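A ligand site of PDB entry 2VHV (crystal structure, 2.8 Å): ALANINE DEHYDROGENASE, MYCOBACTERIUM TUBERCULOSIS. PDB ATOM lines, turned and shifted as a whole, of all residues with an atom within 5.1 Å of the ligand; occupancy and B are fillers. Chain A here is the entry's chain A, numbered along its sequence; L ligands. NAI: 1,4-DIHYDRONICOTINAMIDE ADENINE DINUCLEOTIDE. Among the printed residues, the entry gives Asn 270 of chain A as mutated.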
ATOM      1  N   HIS A  96      -8.311 -25.664  14.114  1.00  0.00           N
ATOM      2  CA  HIS A  96      -8.902 -24.717  15.068  1.00  0.00           C
ATOM      3  C   HIS A  96      -7.987 -23.539  15.395  1.00  0.00           C
ATOM      4  O   HIS A  96      -7.740 -23.229  16.570  1.00  0.00           O
ATOM      5  CB  HIS A  96      -9.307 -25.437  16.358  1.00  0.00           C
ATOM      6  CG  HIS A  96      -9.986 -26.751  16.134  1.00  0.00           C
ATOM      7  ND1 HIS A  96     -11.259 -26.848  15.630  1.00  0.00           N
ATOM      8  CD2 HIS A  96      -9.562 -28.011  16.359  1.00  0.00           C
ATOM      9  CE1 HIS A  96     -11.586 -28.124  15.538  1.00  0.00           C
ATOM     10  NE2 HIS A  96     -10.585 -28.852  15.983  1.00  0.00           N
ATOM     11  N   LEU A 130     -16.059 -31.796   9.266  1.00  0.00           N
ATOM     12  CA  LEU A 130     -16.461 -31.492  10.634  1.00  0.00           C
ATOM     13  C   LEU A 130     -17.763 -32.193  11.009  1.00  0.00           C
ATOM     14  O   LEU A 130     -17.938 -32.648  12.134  1.00  0.00           O
ATOM     15  CB  LEU A 130     -16.625 -29.993  10.827  1.00  0.00           C
ATOM     16  CG  LEU A 130     -16.975 -29.645  12.277  1.00  0.00           C
ATOM     17  CD1 LEU A 130     -15.730 -29.783  13.159  1.00  0.00           C
ATOM     18  CD2 LEU A 130     -17.595 -28.262  12.388  1.00  0.00           C
ATOM     19  N   MET A 133     -17.979 -35.206  13.217  1.00  0.00           N
ATOM     20  CA  MET A 133     -17.408 -34.999  14.543  1.00  0.00           C
ATOM     21  C   MET A 133     -18.381 -34.199  15.374  1.00  0.00           C
ATOM     22  O   MET A 133     -18.537 -34.471  16.560  1.00  0.00           O
ATOM     23  CB  MET A 133     -16.010 -34.403  14.503  1.00  0.00           C
ATOM     24  CG  MET A 133     -14.952 -35.363  13.918  1.00  0.00           C
ATOM     25  SD  MET A 133     -14.854 -37.012  14.691  1.00  0.00           S
ATOM     26  CE  MET A 133     -15.918 -38.010  13.670  1.00  0.00           C
ATOM     27  N   SER A 134     -19.087 -33.268  14.727  1.00  0.00           N
ATOM     28  CA  SER A 134     -20.177 -32.556  15.377  1.00  0.00           C
ATOM     29  C   SER A 134     -21.270 -33.525  15.794  1.00  0.00           C
ATOM     30  O   SER A 134     -21.790 -33.432  16.904  1.00  0.00           O
ATOM     31  CB  SER A 134     -20.750 -31.496  14.453  1.00  0.00           C
ATOM     32  OG  SER A 134     -19.792 -30.490  14.226  1.00  0.00           O
ATOM     33  N   ALA A 137     -20.001 -35.298  18.792  1.00  0.00           N
ATOM     34  CA  ALA A 137     -19.944 -34.371  19.908  1.00  0.00           C
ATOM     35  C   ALA A 137     -21.346 -34.064  20.487  1.00  0.00           C
ATOM     36  O   ALA A 137     -21.549 -34.145  21.701  1.00  0.00           O
ATOM     37  CB  ALA A 137     -19.197 -33.101  19.537  1.00  0.00           C
ATOM     38  N   ILE A 174     -27.867 -24.334  22.527  1.00  0.00           N
ATOM     39  CA  ILE A 174     -27.640 -23.080  21.836  1.00  0.00           C
ATOM     40  C   ILE A 174     -26.970 -23.391  20.501  1.00  0.00           C
ATOM     41  O   ILE A 174     -25.763 -23.687  20.465  1.00  0.00           O
ATOM     42  CB  ILE A 174     -26.752 -22.130  22.682  1.00  0.00           C
ATOM     43  CG1 ILE A 174     -27.351 -21.965  24.094  1.00  0.00           C
ATOM     44  CG2 ILE A 174     -26.557 -20.797  21.982  1.00  0.00           C
ATOM     45  CD1 ILE A 174     -26.485 -21.200  25.072  1.00  0.00           C
ATOM     46  N   GLY A 175     -27.766 -23.359  19.439  1.00  0.00           N
ATOM     47  CA  GLY A 175     -27.277 -23.641  18.109  1.00  0.00           C
ATOM     48  C   GLY A 175     -28.001 -24.858  17.564  1.00  0.00           C
ATOM     49  O   GLY A 175     -28.031 -25.902  18.218  1.00  0.00           O
ATOM     50  N   ALA A 176     -28.574 -24.720  16.366  1.00  0.00           N
ATOM     51  CA  ALA A 176     -29.370 -25.770  15.743  1.00  0.00           C
ATOM     52  C   ALA A 176     -28.624 -26.455  14.585  1.00  0.00           C
ATOM     53  O   ALA A 176     -29.245 -27.034  13.696  1.00  0.00           O
ATOM     54  CB  ALA A 176     -30.673 -25.177  15.235  1.00  0.00           C
ATOM     55  N   GLY A 177     -27.291 -26.368  14.586  1.00  0.00           N
ATOM     56  CA  GLY A 177     -26.483 -26.948  13.516  1.00  0.00           C
ATOM     57  C   GLY A 177     -26.369 -28.462  13.694  1.00  0.00           C
ATOM     58  O   GLY A 177     -27.295 -29.115  14.216  1.00  0.00           O
ATOM     59  N   THR A 178     -25.245 -29.023  13.286  1.00  0.00           N
ATOM     60  CA  THR A 178     -25.066 -30.458  13.422  1.00  0.00           C
ATOM     61  C   THR A 178     -24.940 -30.878  14.887  1.00  0.00           C
ATOM     62  O   THR A 178     -25.635 -31.784  15.336  1.00  0.00           O
ATOM     63  CB  THR A 178     -23.858 -30.966  12.605  1.00  0.00           C
ATOM     64  OG1 THR A 178     -23.922 -30.410  11.287  1.00  0.00           O
ATOM     65  CG2 THR A 178     -23.895 -32.462  12.501  1.00  0.00           C
ATOM     66  N   ALA A 179     -24.045 -30.232  15.644  1.00  0.00           N
ATOM     67  CA  ALA A 179     -23.811 -30.655  17.023  1.00  0.00           C
ATOM     68  C   ALA A 179     -25.113 -30.489  17.816  1.00  0.00           C
ATOM     69  O   ALA A 179     -25.563 -31.424  18.495  1.00  0.00           O
ATOM     70  CB  ALA A 179     -22.683 -29.883  17.640  1.00  0.00           C
ATOM     71  N   GLY A 180     -25.729 -29.317  17.662  1.00  0.00           N
ATOM     72  CA  GLY A 180     -26.888 -28.939  18.467  1.00  0.00           C
ATOM     73  C   GLY A 180     -28.107 -29.759  18.137  1.00  0.00           C
ATOM     74  O   GLY A 180     -28.850 -30.117  19.025  1.00  0.00           O
ATOM     75  N   LEU A 197     -32.091 -22.890  20.636  1.00  0.00           N
ATOM     76  CA  LEU A 197     -32.064 -21.508  20.170  1.00  0.00           C
ATOM     77  C   LEU A 197     -31.129 -21.372  18.992  1.00  0.00           C
ATOM     78  O   LEU A 197     -30.213 -22.164  18.835  1.00  0.00           O
ATOM     79  CB  LEU A 197     -31.662 -20.559  21.297  1.00  0.00           C
ATOM     80  CG  LEU A 197     -32.582 -20.574  22.509  1.00  0.00           C
ATOM     81  CD1 LEU A 197     -31.973 -21.367  23.609  1.00  0.00           C
ATOM     82  CD2 LEU A 197     -32.844 -19.184  23.004  1.00  0.00           C
ATOM     83  N   ASP A 198     -31.379 -20.397  18.148  1.00  0.00           N
ATOM     84  CA  ASP A 198     -30.520 -20.149  17.005  1.00  0.00           C
ATOM     85  C   ASP A 198     -30.903 -18.826  16.357  1.00  0.00           C
ATOM     86  O   ASP A 198     -32.040 -18.408  16.450  1.00  0.00           O
ATOM     87  CB  ASP A 198     -30.632 -21.282  15.997  1.00  0.00           C
ATOM     88  CG  ASP A 198     -29.443 -21.325  15.053  1.00  0.00           C
ATOM     89  OD1 ASP A 198     -29.245 -20.334  14.296  1.00  0.00           O
ATOM     90  OD2 ASP A 198     -28.718 -22.353  15.044  1.00  0.00           O
ATOM     91  N   ILE A 199     -29.943 -18.168  15.709  1.00  0.00           N
ATOM     92  CA  ILE A 199     -30.273 -16.927  15.007  1.00  0.00           C
ATOM     93  C   ILE A 199     -30.749 -17.189  13.569  1.00  0.00           C
ATOM     94  O   ILE A 199     -31.103 -16.259  12.842  1.00  0.00           O
ATOM     95  CB  ILE A 199     -29.159 -15.827  15.097  1.00  0.00           C
ATOM     96  CG1 ILE A 199     -27.774 -16.365  14.752  1.00  0.00           C
ATOM     97  CG2 ILE A 199     -29.143 -15.219  16.495  1.00  0.00           C
ATOM     98  CD1 ILE A 199     -27.312 -15.979  13.367  1.00  0.00           C
ATOM     99  N   ASN A 200     -30.776 -18.466  13.171  1.00  0.00           N
ATOM    100  CA  ASN A 200     -31.235 -18.833  11.846  1.00  0.00           C
ATOM    101  C   ASN A 200     -32.566 -19.566  11.943  1.00  0.00           C
ATOM    102  O   ASN A 200     -32.613 -20.754  12.262  1.00  0.00           O
ATOM    103  CB  ASN A 200     -30.164 -19.667  11.143  1.00  0.00           C
ATOM    104  CG  ASN A 200     -30.575 -20.087   9.733  1.00  0.00           C
ATOM    105  OD1 ASN A 200     -31.714 -19.890   9.319  1.00  0.00           O
ATOM    106  ND2 ASN A 200     -29.649 -20.683   9.001  1.00  0.00           N
ATOM    107  N   LYS A 203     -33.141 -23.140  10.536  1.00  0.00           N
ATOM    108  CA  LYS A 203     -32.663 -24.215  11.352  1.00  0.00           C
ATOM    109  C   LYS A 203     -33.711 -24.668  12.378  1.00  0.00           C
ATOM    110  O   LYS A 203     -33.862 -25.861  12.600  1.00  0.00           O
ATOM    111  CB  LYS A 203     -31.350 -23.811  11.999  1.00  0.00           C
ATOM    112  CG  LYS A 203     -30.099 -24.500  11.417  1.00  0.00           C
ATOM    113  CD  LYS A 203     -29.759 -23.984  10.033  1.00  0.00           C
ATOM    114  CE  LYS A 203     -28.422 -24.538   9.565  1.00  0.00           C
ATOM    115  NZ  LYS A 203     -27.259 -24.049  10.361  1.00  0.00           N
ATOM    116  N   SER A 220     -33.073 -17.031  19.146  1.00  0.00           N
ATOM    117  CA  SER A 220     -31.971 -16.600  20.013  1.00  0.00           C
ATOM    118  C   SER A 220     -31.792 -15.073  20.127  1.00  0.00           C
ATOM    119  O   SER A 220     -30.778 -14.515  19.718  1.00  0.00           O
ATOM    120  CB  SER A 220     -30.698 -17.235  19.517  1.00  0.00           C
ATOM    121  OG  SER A 220     -29.734 -17.178  20.551  1.00  0.00           O
ATOM    122  N   ALA A 238     -23.339 -24.911  21.336  1.00  0.00           N
ATOM    123  CA  ALA A 238     -23.078 -25.533  20.042  1.00  0.00           C
ATOM    124  C   ALA A 238     -23.163 -24.561  18.861  1.00  0.00           C
ATOM    125  O   ALA A 238     -23.773 -24.887  17.828  1.00  0.00           O
ATOM    126  CB  ALA A 238     -24.036 -26.707  19.842  1.00  0.00           C
ATOM    127  N   VAL A 239     -22.531 -23.403  18.966  1.00  0.00           N
ATOM    128  CA  VAL A 239     -22.582 -22.427  17.881  1.00  0.00           C
ATOM    129  C   VAL A 239     -21.305 -22.394  17.053  1.00  0.00           C
ATOM    130  O   VAL A 239     -20.244 -22.862  17.489  1.00  0.00           O
ATOM    131  CB  VAL A 239     -22.902 -21.016  18.393  1.00  0.00           C
ATOM    132  CG1 VAL A 239     -24.274 -20.996  19.051  1.00  0.00           C
ATOM    133  CG2 VAL A 239     -21.819 -20.532  19.342  1.00  0.00           C
ATOM    134  N   LEU A 240     -21.415 -21.874  15.834  1.00  0.00           N
ATOM    135  CA  LEU A 240     -20.283 -21.837  14.915  1.00  0.00           C
ATOM    136  C   LEU A 240     -20.548 -20.925  13.742  1.00  0.00           C
ATOM    137  O   LEU A 240     -21.607 -20.986  13.105  1.00  0.00           O
ATOM    138  CB  LEU A 240     -19.959 -23.229  14.351  1.00  0.00           C
ATOM    139  CG  LEU A 240     -18.796 -23.294  13.361  1.00  0.00           C
ATOM    140  CD1 LEU A 240     -17.479 -23.327  14.107  1.00  0.00           C
ATOM    141  CD2 LEU A 240     -18.889 -24.484  12.423  1.00  0.00           C
ATOM    142  N   VAL A 241     -19.575 -20.060  13.477  1.00  0.00           N
ATOM    143  CA  VAL A 241     -19.394 -19.453  12.173  1.00  0.00           C
ATOM    144  C   VAL A 241     -18.150 -20.170  11.623  1.00  0.00           C
ATOM    145  O   VAL A 241     -17.097 -20.157  12.283  1.00  0.00           O
ATOM    146  CB  VAL A 241     -19.174 -17.935  12.291  1.00  0.00           C
ATOM    147  CG1 VAL A 241     -18.652 -17.366  10.981  1.00  0.00           C
ATOM    148  CG2 VAL A 241     -20.467 -17.254  12.718  1.00  0.00           C
ATOM    149  N   PRO A 247     -18.480 -16.904  19.286  1.00  0.00           N
ATOM    150  CA  PRO A 247     -18.988 -15.708  19.975  1.00  0.00           C
ATOM    151  C   PRO A 247     -19.331 -16.041  21.412  1.00  0.00           C
ATOM    152  O   PRO A 247     -19.705 -17.162  21.704  1.00  0.00           O
ATOM    153  CB  PRO A 247     -20.258 -15.355  19.200  1.00  0.00           C
ATOM    154  CG  PRO A 247     -20.740 -16.661  18.655  1.00  0.00           C
ATOM    155  CD  PRO A 247     -19.512 -17.516  18.416  1.00  0.00           C
ATOM    156  N   LEU A 249     -21.732 -16.027  24.226  1.00  0.00           N
ATOM    157  CA  LEU A 249     -23.185 -15.871  24.303  1.00  0.00           C
ATOM    158  C   LEU A 249     -23.743 -16.006  25.722  1.00  0.00           C
ATOM    159  O   LEU A 249     -24.844 -15.539  25.999  1.00  0.00           O
ATOM    160  CB  LEU A 249     -23.874 -16.864  23.360  1.00  0.00           C
ATOM    161  CG  LEU A 249     -23.488 -16.773  21.877  1.00  0.00           C
ATOM    162  CD1 LEU A 249     -24.204 -17.842  21.032  1.00  0.00           C
ATOM    163  CD2 LEU A 249     -23.707 -15.356  21.313  1.00  0.00           C
ATOM    164  N   ILE A 267     -19.633 -27.348  23.715  1.00  0.00           N
ATOM    165  CA  ILE A 267     -19.125 -28.142  22.595  1.00  0.00           C
ATOM    166  C   ILE A 267     -18.179 -27.280  21.779  1.00  0.00           C
ATOM    167  O   ILE A 267     -17.176 -27.768  21.233  1.00  0.00           O
ATOM    168  CB  ILE A 267     -20.264 -28.605  21.683  1.00  0.00           C
ATOM    169  CG1 ILE A 267     -21.304 -29.398  22.479  1.00  0.00           C
ATOM    170  CG2 ILE A 267     -19.725 -29.402  20.498  1.00  0.00           C
ATOM    171  CD1 ILE A 267     -22.435 -29.999  21.623  1.00  0.00           C
ATOM    172  N   ALA A 268     -18.522 -25.993  21.703  1.00  0.00           N
ATOM    173  CA  ALA A 268     -17.798 -25.023  20.883  1.00  0.00           C
ATOM    174  C   ALA A 268     -16.412 -24.672  21.471  1.00  0.00           C
ATOM    175  O   ALA A 268     -15.720 -23.809  20.934  1.00  0.00           O
ATOM    176  CB  ALA A 268     -18.653 -23.764  20.688  1.00  0.00           C
ATOM    177  N   ILE A 269     -16.009 -25.356  22.545  1.00  0.00           N
ATOM    178  CA  ILE A 269     -14.742 -25.032  23.222  1.00  0.00           C
ATOM    179  C   ILE A 269     -13.555 -25.066  22.257  1.00  0.00           C
ATOM    180  O   ILE A 269     -12.709 -24.199  22.304  1.00  0.00           O
ATOM    181  CB  ILE A 269     -14.473 -25.889  24.493  1.00  0.00           C
ATOM    182  CG1 ILE A 269     -13.190 -25.434  25.203  1.00  0.00           C
ATOM    183  CG2 ILE A 269     -14.418 -27.383  24.174  1.00  0.00           C
ATOM    184  CD1 ILE A 269     -13.297 -24.116  25.871  1.00  0.00           C
ATOM    185  N   ASN A 270     -13.541 -26.033  21.356  1.00  0.00           N
ATOM    186  CA  ASN A 270     -12.435 -26.168  20.397  1.00  0.00           C
ATOM    187  C   ASN A 270     -12.218 -24.943  19.487  1.00  0.00           C
ATOM    188  O   ASN A 270     -11.150 -24.802  18.895  1.00  0.00           O
ATOM    189  CB  ASN A 270     -12.595 -27.444  19.553  1.00  0.00           C
ATOM    190  CG  ASN A 270     -13.770 -27.369  18.594  1.00  0.00           C
ATOM    191  OD1 ASN A 270     -14.604 -26.478  18.694  1.00  0.00           O
ATOM    192  ND2 ASN A 270     -13.831 -28.308  17.671  1.00  0.00           N
ATOM    193  N   GLN A 271     -13.234 -24.092  19.372  1.00  0.00           N
ATOM    194  CA  GLN A 271     -13.179 -22.905  18.536  1.00  0.00           C
ATOM    195  C   GLN A 271     -13.237 -21.628  19.401  1.00  0.00           C
ATOM    196  O   GLN A 271     -13.674 -20.568  18.943  1.00  0.00           O
ATOM    197  CB  GLN A 271     -14.331 -22.912  17.527  1.00  0.00           C
ATOM    198  CG  GLN A 271     -14.142 -23.849  16.367  1.00  0.00           C
ATOM    199  CD  GLN A 271     -13.143 -23.335  15.355  1.00  0.00           C
ATOM    200  OE1 GLN A 271     -12.195 -24.046  14.988  1.00  0.00           O
ATOM    201  NE2 GLN A 271     -13.337 -22.104  14.897  1.00  0.00           N
ATOM    202  N   VAL A 298     -14.409 -30.221  26.979  1.00  0.00           N
ATOM    203  CA  VAL A 298     -13.411 -31.063  26.328  1.00  0.00           C
ATOM    204  C   VAL A 298     -13.360 -30.745  24.822  1.00  0.00           C
ATOM    205  O   VAL A 298     -14.378 -30.808  24.119  1.00  0.00           O
ATOM    206  CB  VAL A 298     -13.692 -32.554  26.632  1.00  0.00           C
ATOM    207  CG1 VAL A 298     -12.716 -33.480  25.896  1.00  0.00           C
ATOM    208  CG2 VAL A 298     -13.622 -32.792  28.138  1.00  0.00           C
ATOM    209  N   ALA A 299     -12.176 -30.368  24.336  1.00  0.00           N
ATOM    210  CA  ALA A 299     -12.040 -29.945  22.935  1.00  0.00           C
ATOM    211  C   ALA A 299     -11.904 -31.115  21.974  1.00  0.00           C
ATOM    212  O   ALA A 299     -12.055 -30.935  20.754  1.00  0.00           O
ATOM    213  CB  ALA A 299     -10.879 -29.005  22.782  1.00  0.00           C
ATOM    214  N   ASN A 300     -11.617 -32.302  22.508  1.00  0.00           N
ATOM    215  CA  ASN A 300     -11.603 -33.497  21.687  1.00  0.00           C
ATOM    216  C   ASN A 300     -12.579 -34.563  22.152  1.00  0.00           C
ATOM    217  O   ASN A 300     -12.207 -35.724  22.360  1.00  0.00           O
ATOM    218  CB  ASN A 300     -10.180 -34.056  21.540  1.00  0.00           C
ATOM    219  CG  ASN A 300      -9.615 -34.621  22.828  1.00  0.00           C
ATOM    220  OD1 ASN A 300      -9.924 -34.157  23.934  1.00  0.00           O
ATOM    221  ND2 ASN A 300      -8.756 -35.623  22.698  1.00  0.00           N
ATOM    222  N   MET A 301     -13.851 -34.163  22.294  1.00  0.00           N
ATOM    223  CA  MET A 301     -14.897 -35.047  22.832  1.00  0.00           C
ATOM    224  C   MET A 301     -14.989 -36.398  22.113  1.00  0.00           C
ATOM    225  O   MET A 301     -15.077 -37.432  22.786  1.00  0.00           O
ATOM    226  CB  MET A 301     -16.251 -34.354  22.823  1.00  0.00           C
ATOM    227  CG  MET A 301     -16.404 -33.270  23.881  1.00  0.00           C
ATOM    228  SD  MET A 301     -17.992 -32.414  23.715  1.00  0.00           S
ATOM    229  CE  MET A 301     -19.125 -33.634  24.350  1.00  0.00           C
ATOM    230  N   PRO A 302     -14.957 -36.403  20.765  1.00  0.00           N
ATOM    231  CA  PRO A 302     -15.102 -37.655  20.029  1.00  0.00           C
ATOM    232  C   PRO A 302     -14.071 -38.706  20.402  1.00  0.00           C
ATOM    233  O   PRO A 302     -14.243 -39.872  20.051  1.00  0.00           O
ATOM    234  CB  PRO A 302     -14.894 -37.224  18.567  1.00  0.00           C
ATOM    235  CG  PRO A 302     -15.211 -35.796  18.531  1.00  0.00           C
ATOM    236  CD  PRO A 302     -14.801 -35.249  19.856  1.00  0.00           C
HETATM  237  PA  NAI L   1     -22.971 -25.869  12.561  1.00  0.00           P
HETATM  238  O1A NAI L   1     -22.701 -24.726  11.606  1.00  0.00           O
HETATM  239  O2A NAI L   1     -23.622 -27.152  12.110  1.00  0.00           O
HETATM  240  O5B NAI L   1     -23.928 -25.306  13.724  1.00  0.00           O
HETATM  241  C5B NAI L   1     -23.656 -24.075  14.422  1.00  0.00           C
HETATM  242  C4B NAI L   1     -24.963 -23.303  14.605  1.00  0.00           C
HETATM  243  O4B NAI L   1     -24.772 -22.224  15.523  1.00  0.00           O
HETATM  244  C3B NAI L   1     -25.402 -22.699  13.277  1.00  0.00           C
HETATM  245  O3B NAI L   1     -26.693 -23.230  12.935  1.00  0.00           O
HETATM  246  C2B NAI L   1     -25.437 -21.198  13.523  1.00  0.00           C
HETATM  247  O2B NAI L   1     -26.552 -20.538  12.914  1.00  0.00           O
HETATM  248  C1B NAI L   1     -25.536 -21.106  15.039  1.00  0.00           C
HETATM  249  N9A NAI L   1     -25.092 -19.763  15.527  1.00  0.00           N
HETATM  250  C8A NAI L   1     -24.067 -19.017  15.058  1.00  0.00           C
HETATM  251  N7A NAI L   1     -23.962 -17.848  15.722  1.00  0.00           N
HETATM  252  C5A NAI L   1     -24.944 -17.815  16.637  1.00  0.00           C
HETATM  253  C6A NAI L   1     -25.405 -16.865  17.663  1.00  0.00           C
HETATM  254  N6A NAI L   1     -24.760 -15.693  17.857  1.00  0.00           N
HETATM  255  N1A NAI L   1     -26.479 -17.209  18.426  1.00  0.00           N
HETATM  256  C2A NAI L   1     -27.121 -18.390  18.252  1.00  0.00           C
HETATM  257  N3A NAI L   1     -26.757 -19.297  17.329  1.00  0.00           N
HETATM  258  C4A NAI L   1     -25.690 -19.075  16.512  1.00  0.00           C
HETATM  259  O3  NAI L   1     -21.661 -26.179  13.400  1.00  0.00           O
HETATM  260  PN  NAI L   1     -21.507 -27.579  14.144  1.00  0.00           P
HETATM  261  O1N NAI L   1     -20.938 -28.500  13.102  1.00  0.00           O
HETATM  262  O2N NAI L   1     -22.805 -27.948  14.828  1.00  0.00           O
HETATM  263  O5D NAI L   1     -20.428 -27.227  15.281  1.00  0.00           O
HETATM  264  C5D NAI L   1     -20.703 -26.391  16.407  1.00  0.00           C
HETATM  265  C4D NAI L   1     -19.442 -26.310  17.257  1.00  0.00           C
HETATM  266  O4D NAI L   1     -19.080 -27.599  17.755  1.00  0.00           O
HETATM  267  C3D NAI L   1     -18.229 -25.826  16.469  1.00  0.00           C
HETATM  268  O3D NAI L   1     -17.584 -24.733  17.172  1.00  0.00           O
HETATM  269  C2D NAI L   1     -17.333 -27.056  16.384  1.00  0.00           C
HETATM  270  O2D NAI L   1     -15.946 -26.767  16.197  1.00  0.00           O
HETATM  271  C1D NAI L   1     -17.661 -27.704  17.721  1.00  0.00           C
HETATM  272  N1N NAI L   1     -17.213 -29.089  17.827  1.00  0.00           N
HETATM  273  C2N NAI L   1     -16.568 -29.469  18.964  1.00  0.00           C
HETATM  274  C3N NAI L   1     -16.112 -30.781  19.127  1.00  0.00           C
HETATM  275  C7N NAI L   1     -15.409 -31.247  20.391  1.00  0.00           C
HETATM  276  O7N NAI L   1     -14.831 -32.324  20.415  1.00  0.00           O
HETATM  277  N7N NAI L   1     -15.464 -30.501  21.500  1.00  0.00           N
HETATM  278  C4N NAI L   1     -16.339 -31.695  18.095  1.00  0.00           C
HETATM  279  C5N NAI L   1     -17.017 -31.276  16.940  1.00  0.00           C
HETATM  280  C6N NAI L   1     -17.456 -29.961  16.826  1.00  0.00           C
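O of Ala 299 sits close to O7N of the ligand (3.1 Å). Merely in contact with the ligand: Leu 130, Met 133, Ala 137, Gly 175, Gly 177, Ile 199, Ser 220, Ala 238, Leu 249, Ala 268, Gln 271, Asn 300 and Pro 302. Hydrophobic or aromatic side chains within 4 Å of the ligand: Leu 130, Ala 137, Ala 179, Ile 199, Val 239, Leu 240, Leu 249, Ile 267, Ala 268, Met 301 and Pro 302. Of the 34 residues printed, 25 come within 4 Å of the ligand. The nearest printed residue that does not touch the ligand is Ala 176 (4.1 Å).
A nitrogen (N7N) of the ligand sits at hydrogen-bond distance from the backbone carbonyl oxygen (O) of Val 298 (2.9 Å). O3B of the ligand sits at hydrogen-bond distance from NZ of Lys 203, at 2.8 Å. The backbone NH (N) of Met 301 is in hydrogen-bond range of an oxygen (O7N) of the ligand (2.8 Å). The backbone carbonyl oxygen of Ile 267 sits close to a nitrogen (N7N) of the ligand (3.2 Å). The backbone NH (N) of Leu 240 is in hydrogen-bond range of an oxygen (O4B) of the ligand (3.4 Å). The backbone NH (N) of Thr 178 lies within hydrogen-bond range of an oxygen (O2A) of the ligand (2.7 Å). OD1 of Asp 198 sits at hydrogen-bond distance from O2B of the ligand. The side-chain amide oxygen of Asn 270 sits at hydrogen-bond distance from an oxygen (O2D) of the ligand (2.8 Å). O1N of the ligand is in hydrogen-bond range of OG of Ser 134, 2.6 Å away. OG1 of Thr 178 lies within hydrogen-bond range of O2A of the ligand (3.4 Å). The backbone carbonyl oxygen (O) of Val 239 sits at hydrogen-bond distance from an oxygen (O3D) of the ligand (3.3 Å). O2N of the ligand sits at hydrogen-bond distance from N of Ala 179 (2.7 Å).
The backbone NH (N) of Gly 175 lies within hydrogen-bond range of the backbone carbonyl oxygen (O) of Leu 197, 2.8 Å away. O of Asp 198 lies within hydrogen-bond range of N of Ser 220 (3.2 Å). The backbone carbonyl oxygen (O) of Ile 174 is in hydrogen-bond range of the backbone NH (N) of Ala 238, at 2.9 Å. The side-chain amide oxygen (OE1) of Gln 271 is in hydrogen-bond range of a ring nitrogen (ND1) of His 96, at 3.0 Å. The side-chain carboxylate of Asp 198 is in hydrogen-bond range of the backbone NH of Asn 200 (2.7 Å). The side-chain carboxylate of Asp 198 sits at hydrogen-bond distance from the backbone NH of Ala 176, 2.7 Å away.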
